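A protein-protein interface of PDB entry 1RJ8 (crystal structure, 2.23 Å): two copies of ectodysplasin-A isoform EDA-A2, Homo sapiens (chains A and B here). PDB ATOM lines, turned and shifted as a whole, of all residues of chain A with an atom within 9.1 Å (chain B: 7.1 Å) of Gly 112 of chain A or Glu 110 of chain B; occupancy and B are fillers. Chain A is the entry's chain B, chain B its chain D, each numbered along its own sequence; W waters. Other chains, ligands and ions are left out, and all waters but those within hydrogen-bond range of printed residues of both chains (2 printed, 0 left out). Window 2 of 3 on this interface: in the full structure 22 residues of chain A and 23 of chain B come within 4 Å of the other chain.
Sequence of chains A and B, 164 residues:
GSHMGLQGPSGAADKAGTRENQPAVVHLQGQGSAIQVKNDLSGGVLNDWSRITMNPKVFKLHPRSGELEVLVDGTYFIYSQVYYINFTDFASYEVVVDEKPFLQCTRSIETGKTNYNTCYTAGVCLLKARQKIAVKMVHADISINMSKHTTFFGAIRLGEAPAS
OE1 of Glu 110 of chain A lies within hydrogen-bond range of N of Ser 108 of chain B (2.9 Å). OE2 of Glu 110 of chain A sits at hydrogen-bond distance from ND2 of Asn 115 of chain B (2.8 Å). The side-chain hydroxyl (OG1) of Thr 111 of chain A sits close to the backbone NH (N) of Glu 110 of chain B, at 3.3 Å. The backbone NH (N) of Gly 112 of chain A sits at hydrogen-bond distance from the side-chain carboxylate (OE1) of Glu 110 of chain B, at 3.5 Å.
OD1 of Asn 115 of chain A lies within hydrogen-bond range of N of Glu 110 of chain A (2.9 Å). The side-chain hydroxyl (OG1) of Thr 111 of chain A lies within hydrogen-bond range of the backbone NH (N) of Lys 113 of chain A (3.2 Å). The backbone NH of Thr 111 of chain A is in hydrogen-bond range of the side-chain amide oxygen of Asn 115 of chain A, 3.3 Å away. N of Ile 109 of chain B lies within hydrogen-bond range of O of Asp 89 of chain B (3.1 Å). O of Ser 108 of chain B is in hydrogen-bond range of ND2 of Asn 115 of chain B. OE1 of Glu 110 of chain B lies within salt-bridge range of NZ of Lys 113 of chain B, 3.5 Å away.
Glu 110 of chain A touches Ile 109 of chain B (O to CA, 3.7 Å). Glu 110 of chain A touches Glu 110 of chain B. Thr 111 of chain A touches Ile 109 of chain B (CB to C, 3.6 Å). Ser 108 of chain B touches Thr 114 of chain A (OG to O, 3.8 Å).
Of the printed residues of chain B, Glu 110 of chain A touches Ser 108 (2.9 Å), Ile 109 (3.7 Å), Glu 110 (3.9 Å) and Asn 115 (2.8 Å). Of the printed residues of chain B, Thr 111 of chain A touches Ile 109 and Glu 110. Gly 112 of chain A touches just one residue of chain B: Glu 110. Of the printed residues of chain B, Thr 114 of chain A touches Ser 108 (3.8 Å). Asn 115 of chain A touches none of the printed residues of chain B. Phe 87 of chain B touches none of the printed residues of chain A. Of the printed residues of chain A, Ser 108 of chain B touches Glu 110 and Thr 114. Of chain A, only Glu 110 (3.7 Å) and Thr 111 (3.6 Å) come within 4 Å of Ile 109 of chain B. Glu 110 of chain B touches three residues of chain A. Thr 111 of chain B touches none of the printed residues of chain A. No residue of chain A comes within 4 Å of Lys 113 of chain B. Of the printed residues of chain A, Asn 115 of chain B touches Glu 110 (2.8 Å). The nearest residue of chain B that does not touch Gly 112 of chain A is Ile 109 of chain B (6.3 Å). The nearest printed residue of chain B that does not touch Glu 110 of chain A is Phe 87 of chain B (5.8 Å).
Along chain A the printed residues that touch a printed residue of chain B span positions 110 to 114. Of the 11 printed residues of chain B, 4 touch a printed residue of chain A. Among the printed residues, 8 pairs touch across the chains.
Glu 110 of chain B touches its own counterpart, Glu 110 of chain A. Glu 110 of chain A touches Asn 115 of chain B, but with the chains exchanged Asn 115 of chain A does not touch Glu 110 of chain B (7.4 Å). Thr 111 of chain A touches Ile 109 of chain B, but with the chains exchanged Ile 109 of chain A does not touch Thr 111 of chain B (11.5 Å). Gly 112 of chain A touches Glu 110 of chain B, but with the chains exchanged Glu 110 of chain A does not touch Gly 112 of chain B (9.1 Å). 9 positions are printed for both chains. Of the 8 pairs that touch across the chains among the printed residues, 1 has its exchanged pair printed and touching as well.
Water W1 lies within hydrogen-bond range of the backbone carbonyl oxygen of Ile 109 of chain B and the side-chain hydroxyl of Thr 111 of chain A. Water W2 lies within hydrogen-bond range of O of Glu 110 of chain A (2.7 Å) and N of Glu 110 of chain B (3.4 Å).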
ATOM      1  N   ASN A  86      -6.141  22.122  -0.919  1.00  0.00           N
ATOM      2  CA  ASN A  86      -5.284  23.239  -1.293  1.00  0.00           C
ATOM      3  C   ASN A  86      -5.402  24.368  -0.275  1.00  0.00           C
ATOM      4  O   ASN A  86      -6.500  24.809   0.053  1.00  0.00           O
ATOM      5  CB  ASN A  86      -5.638  23.768  -2.695  1.00  0.00           C
ATOM      6  CG  ASN A  86      -4.547  24.661  -3.288  1.00  0.00           C
ATOM      7  OD1 ASN A  86      -3.376  24.554  -2.937  1.00  0.00           O
ATOM      8  ND2 ASN A  86      -4.936  25.528  -4.214  1.00  0.00           N
ATOM      9  N   PHE A  87      -4.262  24.827   0.218  1.00  0.00           N
ATOM     10  CA  PHE A  87      -4.183  26.027   1.048  1.00  0.00           C
ATOM     11  C   PHE A  87      -2.718  26.308   1.334  1.00  0.00           C
ATOM     12  O   PHE A  87      -1.904  25.384   1.390  1.00  0.00           O
ATOM     13  CB  PHE A  87      -4.995  25.890   2.350  1.00  0.00           C
ATOM     14  CG  PHE A  87      -4.455  24.864   3.308  1.00  0.00           C
ATOM     15  CD1 PHE A  87      -4.817  23.525   3.202  1.00  0.00           C
ATOM     16  CD2 PHE A  87      -3.591  25.239   4.319  1.00  0.00           C
ATOM     17  CE1 PHE A  87      -4.322  22.580   4.089  1.00  0.00           C
ATOM     18  CE2 PHE A  87      -3.083  24.296   5.209  1.00  0.00           C
ATOM     19  CZ  PHE A  87      -3.450  22.963   5.089  1.00  0.00           C
ATOM     20  N   THR A  88      -2.373  27.578   1.489  1.00  0.00           N
ATOM     21  CA  THR A  88      -0.967  27.964   1.626  1.00  0.00           C
ATOM     22  C   THR A  88      -0.604  28.527   2.997  1.00  0.00           C
ATOM     23  O   THR A  88       0.566  28.782   3.268  1.00  0.00           O
ATOM     24  CB  THR A  88      -0.575  28.975   0.523  1.00  0.00           C
ATOM     25  OG1 THR A  88      -1.503  30.068   0.506  1.00  0.00           O
ATOM     26  CG2 THR A  88      -0.680  28.330  -0.881  1.00  0.00           C
ATOM     27  N   ILE A 109       0.340  24.173   7.101  1.00  0.00           N
ATOM     28  CA  ILE A 109       0.840  23.530   5.884  1.00  0.00           C
ATOM     29  C   ILE A 109       1.769  22.372   6.243  1.00  0.00           C
ATOM     30  O   ILE A 109       2.526  22.451   7.215  1.00  0.00           O
ATOM     31  CB  ILE A 109       1.533  24.531   4.908  1.00  0.00           C
ATOM     32  CG1 ILE A 109       2.771  25.184   5.529  1.00  0.00           C
ATOM     33  CG2 ILE A 109       0.544  25.593   4.444  1.00  0.00           C
ATOM     34  CD1 ILE A 109       3.659  25.869   4.517  1.00  0.00           C
ATOM     35  N   GLU A 110       1.665  21.288   5.479  1.00  0.00           N
ATOM     36  CA  GLU A 110       2.595  20.166   5.561  1.00  0.00           C
ATOM     37  C   GLU A 110       3.626  20.210   4.433  1.00  0.00           C
ATOM     38  O   GLU A 110       4.663  19.551   4.513  1.00  0.00           O
ATOM     39  CB  GLU A 110       1.835  18.835   5.520  1.00  0.00           C
ATOM     40  CG  GLU A 110       0.898  18.610   6.701  1.00  0.00           C
ATOM     41  CD  GLU A 110       0.235  17.240   6.691  1.00  0.00           C
ATOM     42  OE1 GLU A 110      -0.619  16.992   5.816  1.00  0.00           O
ATOM     43  OE2 GLU A 110       0.559  16.412   7.569  1.00  0.00           O
ATOM     44  N   THR A 111       3.346  20.983   3.388  1.00  0.00           N
ATOM     45  CA  THR A 111       4.232  21.043   2.225  1.00  0.00           C
ATOM     46  C   THR A 111       4.095  22.355   1.445  1.00  0.00           C
ATOM     47  O   THR A 111       3.063  23.027   1.508  1.00  0.00           O
ATOM     48  CB  THR A 111       3.963  19.818   1.298  1.00  0.00           C
ATOM     49  OG1 THR A 111       4.784  19.886   0.124  1.00  0.00           O
ATOM     50  CG2 THR A 111       2.515  19.803   0.771  1.00  0.00           C
ATOM     51  N   GLY A 112       5.147  22.705   0.715  1.00  0.00           N
ATOM     52  CA  GLY A 112       5.122  23.843  -0.192  1.00  0.00           C
ATOM     53  C   GLY A 112       4.380  23.585  -1.500  1.00  0.00           C
ATOM     54  O   GLY A 112       4.067  24.525  -2.232  1.00  0.00           O
ATOM     55  N   LYS A 113       4.114  22.314  -1.806  1.00  0.00           N
ATOM     56  CA  LYS A 113       3.396  21.937  -3.030  1.00  0.00           C
ATOM     57  C   LYS A 113       1.875  21.947  -2.822  1.00  0.00           C
ATOM     58  O   LYS A 113       1.281  23.026  -2.762  1.00  0.00           O
ATOM     59  CB  LYS A 113       3.893  20.581  -3.546  1.00  0.00           C
ATOM     60  CG  LYS A 113       5.363  20.568  -3.929  1.00  0.00           C
ATOM     61  CD  LYS A 113       5.626  21.406  -5.168  1.00  0.00           C
ATOM     62  CE  LYS A 113       7.082  21.343  -5.568  1.00  0.00           C
ATOM     63  NZ  LYS A 113       7.303  21.980  -6.886  1.00  0.00           N
ATOM     64  N   THR A 114       1.241  20.777  -2.723  1.00  0.00           N
ATOM     65  CA  THR A 114      -0.211  20.704  -2.534  1.00  0.00           C
ATOM     66  C   THR A 114      -0.571  20.022  -1.221  1.00  0.00           C
ATOM     67  O   THR A 114      -0.122  18.917  -0.945  1.00  0.00           O
ATOM     68  CB  THR A 114      -0.891  19.950  -3.707  1.00  0.00           C
ATOM     69  OG1 THR A 114      -0.629  20.622  -4.943  1.00  0.00           O
ATOM     70  CG2 THR A 114      -2.417  20.009  -3.588  1.00  0.00           C
ATOM     71  N   ASN A 115      -1.425  20.672  -0.440  1.00  0.00           N
ATOM     72  CA  ASN A 115      -1.765  20.216   0.896  1.00  0.00           C
ATOM     73  C   ASN A 115      -3.036  19.356   0.907  1.00  0.00           C
ATOM     74  O   ASN A 115      -4.150  19.865   1.061  1.00  0.00           O
ATOM     75  CB  ASN A 115      -1.903  21.418   1.830  1.00  0.00           C
ATOM     76  CG  ASN A 115      -0.559  21.945   2.297  1.00  0.00           C
ATOM     77  OD1 ASN A 115       0.126  21.290   3.068  1.00  0.00           O
ATOM     78  ND2 ASN A 115      -0.178  23.129   1.832  1.00  0.00           N
ATOM     79  N   PHE B  87       6.964   8.874   4.684  1.00  0.00           N
ATOM     80  CA  PHE B  87       6.459   8.584   3.334  1.00  0.00           C
ATOM     81  C   PHE B  87       6.863   9.644   2.303  1.00  0.00           C
ATOM     82  O   PHE B  87       7.285  10.746   2.657  1.00  0.00           O
ATOM     83  CB  PHE B  87       4.936   8.423   3.335  1.00  0.00           C
ATOM     84  CG  PHE B  87       4.182   9.632   3.823  1.00  0.00           C
ATOM     85  CD1 PHE B  87       3.885   9.784   5.169  1.00  0.00           C
ATOM     86  CD2 PHE B  87       3.739  10.598   2.928  1.00  0.00           C
ATOM     87  CE1 PHE B  87       3.172  10.886   5.618  1.00  0.00           C
ATOM     88  CE2 PHE B  87       3.026  11.703   3.365  1.00  0.00           C
ATOM     89  CZ  PHE B  87       2.739  11.850   4.714  1.00  0.00           C
ATOM     90  N   THR B  88       6.713   9.312   1.024  1.00  0.00           N
ATOM     91  CA  THR B  88       7.218  10.163  -0.059  1.00  0.00           C
ATOM     92  C   THR B  88       6.584  11.553  -0.110  1.00  0.00           C
ATOM     93  O   THR B  88       7.279  12.560   0.020  1.00  0.00           O
ATOM     94  CB  THR B  88       7.028   9.473  -1.424  1.00  0.00           C
ATOM     95  OG1 THR B  88       7.956   8.386  -1.560  1.00  0.00           O
ATOM     96  CG2 THR B  88       7.391  10.420  -2.574  1.00  0.00           C
ATOM     97  N   ASP B  89       5.275  11.594  -0.325  1.00  0.00           N
ATOM     98  CA  ASP B  89       4.559  12.855  -0.515  1.00  0.00           C
ATOM     99  C   ASP B  89       3.065  12.805  -0.198  1.00  0.00           C
ATOM    100  O   ASP B  89       2.488  13.803   0.210  1.00  0.00           O
ATOM    101  CB  ASP B  89       4.766  13.371  -1.943  1.00  0.00           C
ATOM    102  CG  ASP B  89       4.312  12.384  -3.004  1.00  0.00           C
ATOM    103  OD1 ASP B  89       3.867  11.266  -2.664  1.00  0.00           O
ATOM    104  OD2 ASP B  89       4.382  12.646  -4.222  1.00  0.00           O
ATOM    105  N   SER B 108      -0.082  14.812   3.949  1.00  0.00           N
ATOM    106  CA  SER B 108       0.841  15.208   2.896  1.00  0.00           C
ATOM    107  C   SER B 108       2.206  15.590   3.460  1.00  0.00           C
ATOM    108  O   SER B 108       2.374  15.810   4.662  1.00  0.00           O
ATOM    109  CB  SER B 108       0.273  16.387   2.109  1.00  0.00           C
ATOM    110  OG  SER B 108      -0.858  15.994   1.363  1.00  0.00           O
ATOM    111  N   ILE B 109       3.174  15.680   2.560  1.00  0.00           N
ATOM    112  CA  ILE B 109       4.492  16.193   2.892  1.00  0.00           C
ATOM    113  C   ILE B 109       5.300  16.468   1.629  1.00  0.00           C
ATOM    114  O   ILE B 109       5.054  15.867   0.578  1.00  0.00           O
ATOM    115  CB  ILE B 109       5.251  15.215   3.803  1.00  0.00           C
ATOM    116  CG1 ILE B 109       6.541  15.871   4.273  1.00  0.00           C
ATOM    117  CG2 ILE B 109       5.527  13.904   3.072  1.00  0.00           C
ATOM    118  CD1 ILE B 109       7.143  15.216   5.371  1.00  0.00           C
ATOM    119  N   GLU B 110       6.257  17.382   1.738  1.00  0.00           N
ATOM    120  CA  GLU B 110       7.143  17.687   0.626  1.00  0.00           C
ATOM    121  C   GLU B 110       8.143  16.545   0.441  1.00  0.00           C
ATOM    122  O   GLU B 110       8.666  15.993   1.414  1.00  0.00           O
ATOM    123  CB  GLU B 110       7.857  19.030   0.828  1.00  0.00           C
ATOM    124  CG  GLU B 110       8.123  19.747  -0.491  1.00  0.00           C
ATOM    125  CD  GLU B 110       8.325  21.243  -0.351  1.00  0.00           C
ATOM    126  OE1 GLU B 110       8.467  21.750   0.784  1.00  0.00           O
ATOM    127  OE2 GLU B 110       8.346  21.917  -1.400  1.00  0.00           O
ATOM    128  N   THR B 111       8.403  16.212  -0.819  1.00  0.00           N
ATOM    129  CA  THR B 111       9.064  14.959  -1.190  1.00  0.00           C
ATOM    130  C   THR B 111      10.157  14.490  -0.216  1.00  0.00           C
ATOM    131  O   THR B 111       9.999  13.459   0.453  1.00  0.00           O
ATOM    132  CB  THR B 111       9.611  15.054  -2.628  1.00  0.00           C
ATOM    133  OG1 THR B 111       8.515  15.190  -3.542  1.00  0.00           O
ATOM    134  CG2 THR B 111      10.266  13.753  -3.068  1.00  0.00           C
ATOM    135  N   GLY B 112      11.238  15.253  -0.114  1.00  0.00           N
ATOM    136  CA  GLY B 112      12.402  14.824   0.642  1.00  0.00           C
ATOM    137  C   GLY B 112      12.341  14.903   2.163  1.00  0.00           C
ATOM    138  O   GLY B 112      13.330  14.608   2.830  1.00  0.00           O
ATOM    139  N   LYS B 113      11.199  15.298   2.720  1.00  0.00           N
ATOM    140  CA  LYS B 113      11.060  15.516   4.158  1.00  0.00           C
ATOM    141  C   LYS B 113      10.167  14.450   4.814  1.00  0.00           C
ATOM    142  O   LYS B 113       9.517  13.660   4.121  1.00  0.00           O
ATOM    143  CB  LYS B 113      10.512  16.924   4.413  1.00  0.00           C
ATOM    144  CG  LYS B 113      11.458  18.039   3.961  1.00  0.00           C
ATOM    145  CD  LYS B 113      10.803  19.418   4.010  1.00  0.00           C
ATOM    146  CE  LYS B 113      11.569  20.437   3.162  1.00  0.00           C
ATOM    147  NZ  LYS B 113      10.949  21.791   3.211  1.00  0.00           N
ATOM    148  N   THR B 114      10.130  14.451   6.149  1.00  0.00           N
ATOM    149  CA  THR B 114       9.490  13.384   6.941  1.00  0.00           C
ATOM    150  C   THR B 114       8.231  13.829   7.675  1.00  0.00           C
ATOM    151  O   THR B 114       8.147  14.958   8.159  1.00  0.00           O
ATOM    152  CB  THR B 114      10.466  12.835   7.993  1.00  0.00           C
ATOM    153  OG1 THR B 114      10.990  13.912   8.788  1.00  0.00           O
ATOM    154  CG2 THR B 114      11.686  12.190   7.332  1.00  0.00           C
ATOM    155  N   ASN B 115       7.260  12.921   7.755  1.00  0.00           N
ATOM    156  CA  ASN B 115       5.994  13.170   8.435  1.00  0.00           C
ATOM    157  C   ASN B 115       5.564  11.940   9.242  1.00  0.00           C
ATOM    158  O   ASN B 115       5.150  10.925   8.678  1.00  0.00           O
ATOM    159  CB  ASN B 115       4.912  13.540   7.413  1.00  0.00           C
ATOM    160  CG  ASN B 115       3.708  14.228   8.041  1.00  0.00           C
ATOM    161  OD1 ASN B 115       3.463  14.119   9.237  1.00  0.00           O
ATOM    162  ND2 ASN B 115       2.942  14.934   7.218  1.00  0.00           N
HETATM  163  O   HOH W   1       4.381  17.570  -1.391  1.00  0.00           O
HETATM  164  O   HOH W   2       7.376  19.439   4.191  1.00  0.00           O
